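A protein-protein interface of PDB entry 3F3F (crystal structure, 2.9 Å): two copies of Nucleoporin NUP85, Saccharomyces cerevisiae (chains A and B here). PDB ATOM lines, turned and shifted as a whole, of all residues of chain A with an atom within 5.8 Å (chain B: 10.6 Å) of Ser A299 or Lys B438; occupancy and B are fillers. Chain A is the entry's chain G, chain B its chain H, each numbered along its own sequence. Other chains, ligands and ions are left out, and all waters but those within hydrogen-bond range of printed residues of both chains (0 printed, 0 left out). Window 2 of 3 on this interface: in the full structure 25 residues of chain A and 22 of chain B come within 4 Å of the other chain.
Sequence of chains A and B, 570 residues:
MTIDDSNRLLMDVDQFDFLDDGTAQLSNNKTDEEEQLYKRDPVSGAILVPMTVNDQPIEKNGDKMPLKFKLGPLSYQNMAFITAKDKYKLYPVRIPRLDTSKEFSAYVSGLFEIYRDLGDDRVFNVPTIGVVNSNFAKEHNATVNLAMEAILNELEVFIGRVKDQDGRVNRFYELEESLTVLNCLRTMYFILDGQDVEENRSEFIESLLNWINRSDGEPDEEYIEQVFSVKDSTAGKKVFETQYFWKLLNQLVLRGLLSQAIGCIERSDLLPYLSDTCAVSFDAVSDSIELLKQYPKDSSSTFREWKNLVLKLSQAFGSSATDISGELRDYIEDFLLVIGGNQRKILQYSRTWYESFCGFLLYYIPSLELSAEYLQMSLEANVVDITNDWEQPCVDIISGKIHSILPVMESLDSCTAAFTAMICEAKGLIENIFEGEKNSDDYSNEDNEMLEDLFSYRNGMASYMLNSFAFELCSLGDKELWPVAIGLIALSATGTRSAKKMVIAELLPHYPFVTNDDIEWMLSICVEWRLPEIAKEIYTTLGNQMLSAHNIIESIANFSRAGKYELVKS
Of the printed residues of chain B, Glu A198 touches Gly B436, Glu B437 and Lys B438.
No residue of chain B comes within 4 Å of Pro A296.
Ser A299 touches just one residue of chain B: Lys B438.
Ser A301 touches just one residue of chain B: Lys B438.
Of the printed residues of chain B, Arg A304 touches Glu B437 and Leu B451.
Of the printed residues of chain A, Gly B436 touches Glu A198 (3.0 Å).
Of the printed residues of chain A, Glu B437 touches Glu A198 (3.0 Å) and Arg A304 (3.1 Å).
Printed residues of chain A within 4 Å of Lys B438: Glu A198, Ser A299 and Ser A301.
The nearest printed residue of chain A that does not touch Glu B437 is Ser A301 (6.4 Å).
Among the printed residues, merely in contact across the chains: Glu A198 with Glu B437 (3.0 Å), Glu A198 with Lys B438 (3.99 Å), Ser A299 with Lys B438 (3.6 Å), Ser A301 with Lys B438 (3.7 Å) and Arg A304 with Leu B451 (3.6 Å).
The guanidinium group (NH1) of Arg A304 is in salt-bridge range of the side-chain carboxylate (OE1) of Glu B437, at 3.1 Å.
The side-chain carboxylate (OE1) of Glu A198 lies close to the backbone carbonyl oxygen (O) of Gly B436, at 3.0 Å.
Of the 9 printed residues of chain B, 4 touch a printed residue of chain A.
Hydrophobic or aromatic side chains of chain B within 4 Å of the printed part of chain A: Leu B451.
Along chain B the printed residues that touch a printed residue of chain A span positions 436 to 451.
Along chain A the printed residues that touch a printed residue of chain B span positions 198 to 304.
Among the printed residues, 7 pairs touch across the chains.
Among the printed residues, Asp or Glu carboxylates within 4 Å of a Lys or Arg side-chain nitrogen of the other chain: Arg A304 with Glu B437 (3.1 Å).
No position is printed for both chains.
The side-chain hydroxyl (OG) of Ser A301 sits close to the side-chain hydroxyl (OG) of Ser A299 (3.2 Å).
OG of Ser A299 lies close to OG1 of Thr A302, 3.5 Å away.
The side-chain carboxylate (OE2) of Glu B437 is in salt-bridge range of the guanidinium group (NH2) of Arg B458 (3.8 Å).
O of Leu B451 sits at hydrogen-bond distance from NH1 of Arg B458, 2.4 Å away.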
ATOM      1  N   GLU A 198      -3.170  21.155 -23.955  1.00  0.00           N
ATOM      2  CA  GLU A 198      -2.296  22.316 -24.060  1.00  0.00           C
ATOM      3  C   GLU A 198      -0.831  21.953 -23.926  1.00  0.00           C
ATOM      4  O   GLU A 198       0.029  22.603 -24.508  1.00  0.00           O
ATOM      5  CB  GLU A 198      -2.683  23.397 -23.060  1.00  0.00           C
ATOM      6  CG  GLU A 198      -3.402  24.514 -23.786  1.00  0.00           C
ATOM      7  CD  GLU A 198      -3.314  25.851 -23.099  1.00  0.00           C
ATOM      8  OE1 GLU A 198      -2.190  26.251 -22.716  1.00  0.00           O
ATOM      9  OE2 GLU A 198      -4.372  26.511 -22.965  1.00  0.00           O
ATOM     10  N   ARG A 201      -0.394  20.492 -28.037  1.00  0.00           N
ATOM     11  CA  ARG A 201      -1.467  20.495 -29.020  1.00  0.00           C
ATOM     12  C   ARG A 201      -1.117  19.850 -30.361  1.00  0.00           C
ATOM     13  O   ARG A 201      -1.923  19.122 -30.929  1.00  0.00           O
ATOM     14  CB  ARG A 201      -1.969  21.922 -29.266  1.00  0.00           C
ATOM     15  CG  ARG A 201      -3.280  21.956 -30.045  1.00  0.00           C
ATOM     16  CD  ARG A 201      -3.649  23.329 -30.559  1.00  0.00           C
ATOM     17  NE  ARG A 201      -4.830  23.267 -31.413  1.00  0.00           N
ATOM     18  CZ  ARG A 201      -6.058  22.994 -30.979  1.00  0.00           C
ATOM     19  NH1 ARG A 201      -6.277  22.758 -29.695  1.00  0.00           N
ATOM     20  NH2 ARG A 201      -7.070  22.946 -31.833  1.00  0.00           N
ATOM     21  N   PRO A 296      -5.580  26.281 -36.201  1.00  0.00           N
ATOM     22  CA  PRO A 296      -4.374  26.067 -35.387  1.00  0.00           C
ATOM     23  C   PRO A 296      -4.124  24.620 -34.985  1.00  0.00           C
ATOM     24  O   PRO A 296      -5.037  23.918 -34.561  1.00  0.00           O
ATOM     25  CB  PRO A 296      -4.615  26.947 -34.166  1.00  0.00           C
ATOM     26  CG  PRO A 296      -5.564  27.995 -34.670  1.00  0.00           C
ATOM     27  CD  PRO A 296      -6.499  27.214 -35.532  1.00  0.00           C
ATOM     28  N   LYS A 297      -2.886  24.170 -35.109  1.00  0.00           N
ATOM     29  CA  LYS A 297      -2.561  22.809 -34.731  1.00  0.00           C
ATOM     30  C   LYS A 297      -1.297  22.760 -33.904  1.00  0.00           C
ATOM     31  O   LYS A 297      -0.758  21.683 -33.684  1.00  0.00           O
ATOM     32  CB  LYS A 297      -2.382  21.934 -35.970  1.00  0.00           C
ATOM     33  CG  LYS A 297      -3.676  21.592 -36.681  1.00  0.00           C
ATOM     34  CD  LYS A 297      -3.441  20.769 -37.947  1.00  0.00           C
ATOM     35  CE  LYS A 297      -4.753  20.555 -38.694  1.00  0.00           C
ATOM     36  NZ  LYS A 297      -4.545  19.965 -40.034  1.00  0.00           N
ATOM     37  N   ASP A 298      -0.819  23.912 -33.441  1.00  0.00           N
ATOM     38  CA  ASP A 298       0.406  23.946 -32.643  1.00  0.00           C
ATOM     39  C   ASP A 298       0.287  24.779 -31.384  1.00  0.00           C
ATOM     40  O   ASP A 298       0.804  24.403 -30.333  1.00  0.00           O
ATOM     41  CB  ASP A 298       1.566  24.473 -33.483  1.00  0.00           C
ATOM     42  CG  ASP A 298       1.791  23.648 -34.736  1.00  0.00           C
ATOM     43  OD1 ASP A 298       0.973  23.761 -35.680  1.00  0.00           O
ATOM     44  OD2 ASP A 298       2.777  22.879 -34.772  1.00  0.00           O
ATOM     45  N   SER A 299      -0.387  25.914 -31.493  1.00  0.00           N
ATOM     46  CA  SER A 299      -0.558  26.780 -30.344  1.00  0.00           C
ATOM     47  C   SER A 299      -2.002  26.744 -29.862  1.00  0.00           C
ATOM     48  O   SER A 299      -2.934  27.002 -30.626  1.00  0.00           O
ATOM     49  CB  SER A 299      -0.156  28.212 -30.702  1.00  0.00           C
ATOM     50  OG  SER A 299      -0.070  29.034 -29.544  1.00  0.00           O
ATOM     51  N   SER A 300      -2.177  26.407 -28.589  1.00  0.00           N
ATOM     52  CA  SER A 300      -3.502  26.350 -27.994  1.00  0.00           C
ATOM     53  C   SER A 300      -3.941  27.787 -27.714  1.00  0.00           C
ATOM     54  O   SER A 300      -5.031  28.041 -27.191  1.00  0.00           O
ATOM     55  CB  SER A 300      -3.458  25.526 -26.703  1.00  0.00           C
ATOM     56  OG  SER A 300      -3.107  24.173 -26.955  1.00  0.00           O
ATOM     57  N   SER A 301      -3.057  28.718 -28.063  1.00  0.00           N
ATOM     58  CA  SER A 301      -3.302  30.147 -27.906  1.00  0.00           C
ATOM     59  C   SER A 301      -3.990  30.547 -29.197  1.00  0.00           C
ATOM     60  O   SER A 301      -5.105  31.071 -29.192  1.00  0.00           O
ATOM     61  CB  SER A 301      -1.984  30.925 -27.796  1.00  0.00           C
ATOM     62  OG  SER A 301      -1.120  30.375 -26.819  1.00  0.00           O
ATOM     63  N   THR A 302      -3.305  30.274 -30.305  1.00  0.00           N
ATOM     64  CA  THR A 302      -3.816  30.583 -31.629  1.00  0.00           C
ATOM     65  C   THR A 302      -5.223  30.014 -31.790  1.00  0.00           C
ATOM     66  O   THR A 302      -6.059  30.605 -32.474  1.00  0.00           O
ATOM     67  CB  THR A 302      -2.898  30.010 -32.716  1.00  0.00           C
ATOM     68  OG1 THR A 302      -1.541  30.337 -32.409  1.00  0.00           O
ATOM     69  CG2 THR A 302      -3.244  30.598 -34.071  1.00  0.00           C
ATOM     70  N   PHE A 303      -5.495  28.874 -31.159  1.00  0.00           N
ATOM     71  CA  PHE A 303      -6.833  28.303 -31.265  1.00  0.00           C
ATOM     72  C   PHE A 303      -7.831  29.140 -30.462  1.00  0.00           C
ATOM     73  O   PHE A 303      -8.956  29.399 -30.903  1.00  0.00           O
ATOM     74  CB  PHE A 303      -6.872  26.848 -30.778  1.00  0.00           C
ATOM     75  CG  PHE A 303      -8.271  26.275 -30.725  1.00  0.00           C
ATOM     76  CD1 PHE A 303      -8.986  26.254 -29.537  1.00  0.00           C
ATOM     77  CD2 PHE A 303      -8.901  25.835 -31.879  1.00  0.00           C
ATOM     78  CE1 PHE A 303     -10.305  25.809 -29.499  1.00  0.00           C
ATOM     79  CE2 PHE A 303     -10.223  25.388 -31.846  1.00  0.00           C
ATOM     80  CZ  PHE A 303     -10.921  25.378 -30.654  1.00  0.00           C
ATOM     81  N   ARG A 304      -7.413  29.565 -29.281  1.00  0.00           N
ATOM     82  CA  ARG A 304      -8.266  30.368 -28.427  1.00  0.00           C
ATOM     83  C   ARG A 304      -8.745  31.585 -29.219  1.00  0.00           C
ATOM     84  O   ARG A 304      -9.914  31.960 -29.150  1.00  0.00           O
ATOM     85  CB  ARG A 304      -7.473  30.796 -27.195  1.00  0.00           C
ATOM     86  CG  ARG A 304      -8.291  31.396 -26.070  1.00  0.00           C
ATOM     87  CD  ARG A 304      -7.364  31.904 -24.964  1.00  0.00           C
ATOM     88  NE  ARG A 304      -8.081  32.643 -23.924  1.00  0.00           N
ATOM     89  CZ  ARG A 304      -7.496  33.298 -22.923  1.00  0.00           C
ATOM     90  NH1 ARG A 304      -6.169  33.313 -22.816  1.00  0.00           N
ATOM     91  NH2 ARG A 304      -8.237  33.940 -22.022  1.00  0.00           N
ATOM     92  N   GLU B 435      -5.908  21.298 -17.415  1.00  0.00           N
ATOM     93  CA  GLU B 435      -4.701  22.104 -17.233  1.00  0.00           C
ATOM     94  C   GLU B 435      -4.769  23.543 -17.771  1.00  0.00           C
ATOM     95  O   GLU B 435      -5.669  23.894 -18.539  1.00  0.00           O
ATOM     96  CB  GLU B 435      -3.493  21.375 -17.828  1.00  0.00           C
ATOM     97  CG  GLU B 435      -2.173  22.015 -17.459  1.00  0.00           C
ATOM     98  CD  GLU B 435      -0.994  21.099 -17.676  1.00  0.00           C
ATOM     99  OE1 GLU B 435      -0.823  20.604 -18.812  1.00  0.00           O
ATOM    100  OE2 GLU B 435      -0.237  20.880 -16.706  1.00  0.00           O
ATOM    101  N   GLY B 436      -3.800  24.362 -17.356  1.00  0.00           N
ATOM    102  CA  GLY B 436      -3.755  25.761 -17.749  1.00  0.00           C
ATOM    103  C   GLY B 436      -3.088  26.150 -19.057  1.00  0.00           C
ATOM    104  O   GLY B 436      -2.935  25.332 -19.963  1.00  0.00           O
ATOM    105  N   GLU B 437      -2.678  27.418 -19.129  1.00  0.00           N
ATOM    106  CA  GLU B 437      -2.049  28.008 -20.315  1.00  0.00           C
ATOM    107  C   GLU B 437      -0.572  28.418 -20.111  1.00  0.00           C
ATOM    108  O   GLU B 437       0.035  28.070 -19.096  1.00  0.00           O
ATOM    109  CB  GLU B 437      -2.882  29.222 -20.736  1.00  0.00           C
ATOM    110  CG  GLU B 437      -4.381  28.941 -20.779  1.00  0.00           C
ATOM    111  CD  GLU B 437      -5.205  30.200 -20.675  1.00  0.00           C
ATOM    112  OE1 GLU B 437      -4.657  31.286 -20.950  1.00  0.00           O
ATOM    113  OE2 GLU B 437      -6.400  30.105 -20.327  1.00  0.00           O
ATOM    114  N   LYS B 438      -0.007  29.155 -21.075  1.00  0.00           N
ATOM    115  CA  LYS B 438       1.393  29.618 -21.022  1.00  0.00           C
ATOM    116  C   LYS B 438       1.732  30.537 -19.836  1.00  0.00           C
ATOM    117  O   LYS B 438       2.347  31.592 -20.024  1.00  0.00           O
ATOM    118  CB  LYS B 438       1.770  30.349 -22.324  1.00  0.00           C
ATOM    119  CG  LYS B 438       1.938  29.464 -23.562  1.00  0.00           C
ATOM    120  CD  LYS B 438       2.195  30.309 -24.818  1.00  0.00           C
ATOM    121  CE  LYS B 438       2.348  29.457 -26.076  1.00  0.00           C
ATOM    122  NZ  LYS B 438       2.505  30.291 -27.304  1.00  0.00           N
ATOM    123  N   ASN B 439       1.332  30.128 -18.629  1.00  0.00           N
ATOM    124  CA  ASN B 439       1.584  30.866 -17.379  1.00  0.00           C
ATOM    125  C   ASN B 439       1.060  32.320 -17.370  1.00  0.00           C
ATOM    126  O   ASN B 439       1.809  33.258 -17.077  1.00  0.00           O
ATOM    127  CB  ASN B 439       3.097  30.819 -17.062  1.00  0.00           C
ATOM    128  CG  ASN B 439       3.434  31.314 -15.656  1.00  0.00           C
ATOM    129  OD1 ASN B 439       2.570  31.383 -14.780  1.00  0.00           O
ATOM    130  ND2 ASN B 439       4.705  31.641 -15.435  1.00  0.00           N
ATOM    131  N   SER B 440      -0.227  32.500 -17.676  1.00  0.00           N
ATOM    132  CA  SER B 440      -0.840  33.832 -17.694  1.00  0.00           C
ATOM    133  C   SER B 440      -1.813  34.016 -16.526  1.00  0.00           C
ATOM    134  O   SER B 440      -3.006  34.267 -16.722  1.00  0.00           O
ATOM    135  CB  SER B 440      -1.580  34.069 -19.017  1.00  0.00           C
ATOM    136  OG  SER B 440      -2.119  35.381 -19.073  1.00  0.00           O
ATOM    137  N   MET B 450     -10.339  37.307 -14.907  1.00  0.00           N
ATOM    138  CA  MET B 450      -9.590  36.398 -15.767  1.00  0.00           C
ATOM    139  C   MET B 450     -10.453  35.155 -15.983  1.00  0.00           C
ATOM    140  O   MET B 450     -11.661  35.262 -16.204  1.00  0.00           O
ATOM    141  CB  MET B 450      -8.255  36.033 -15.093  1.00  0.00           C
ATOM    142  CG  MET B 450      -7.202  35.333 -15.982  1.00  0.00           C
ATOM    143  SD  MET B 450      -6.489  36.304 -17.371  1.00  0.00           S
ATOM    144  CE  MET B 450      -5.373  37.457 -16.536  1.00  0.00           C
ATOM    145  N   LEU B 451      -9.833  33.982 -15.926  1.00  0.00           N
ATOM    146  CA  LEU B 451     -10.552  32.725 -16.094  1.00  0.00           C
ATOM    147  C   LEU B 451     -10.752  32.090 -14.717  1.00  0.00           C
ATOM    148  O   LEU B 451     -10.344  30.956 -14.474  1.00  0.00           O
ATOM    149  CB  LEU B 451      -9.765  31.792 -17.019  1.00  0.00           C
ATOM    150  CG  LEU B 451      -9.949  32.057 -18.513  1.00  0.00           C
ATOM    151  CD1 LEU B 451      -8.708  31.654 -19.284  1.00  0.00           C
ATOM    152  CD2 LEU B 451     -11.179  31.302 -18.997  1.00  0.00           C
ATOM    153  N   ARG B 458     -13.271  23.233 -15.473  1.00  0.00           N
ATOM    154  CA  ARG B 458     -11.850  23.553 -15.388  1.00  0.00           C
ATOM    155  C   ARG B 458     -11.185  22.805 -14.228  1.00  0.00           C
ATOM    156  O   ARG B 458     -10.087  22.263 -14.367  1.00  0.00           O
ATOM    157  CB  ARG B 458     -11.651  25.068 -15.220  1.00  0.00           C
ATOM    158  CG  ARG B 458     -12.132  25.928 -16.391  1.00  0.00           C
ATOM    159  CD  ARG B 458     -11.674  27.379 -16.224  1.00  0.00           C
ATOM    160  NE  ARG B 458     -10.500  27.704 -17.035  1.00  0.00           N
ATOM    161  CZ  ARG B 458      -9.456  28.406 -16.600  1.00  0.00           C
ATOM    162  NH1 ARG B 458      -9.427  28.860 -15.350  1.00  0.00           N
ATOM    163  NH2 ARG B 458      -8.443  28.657 -17.422  1.00  0.00           N
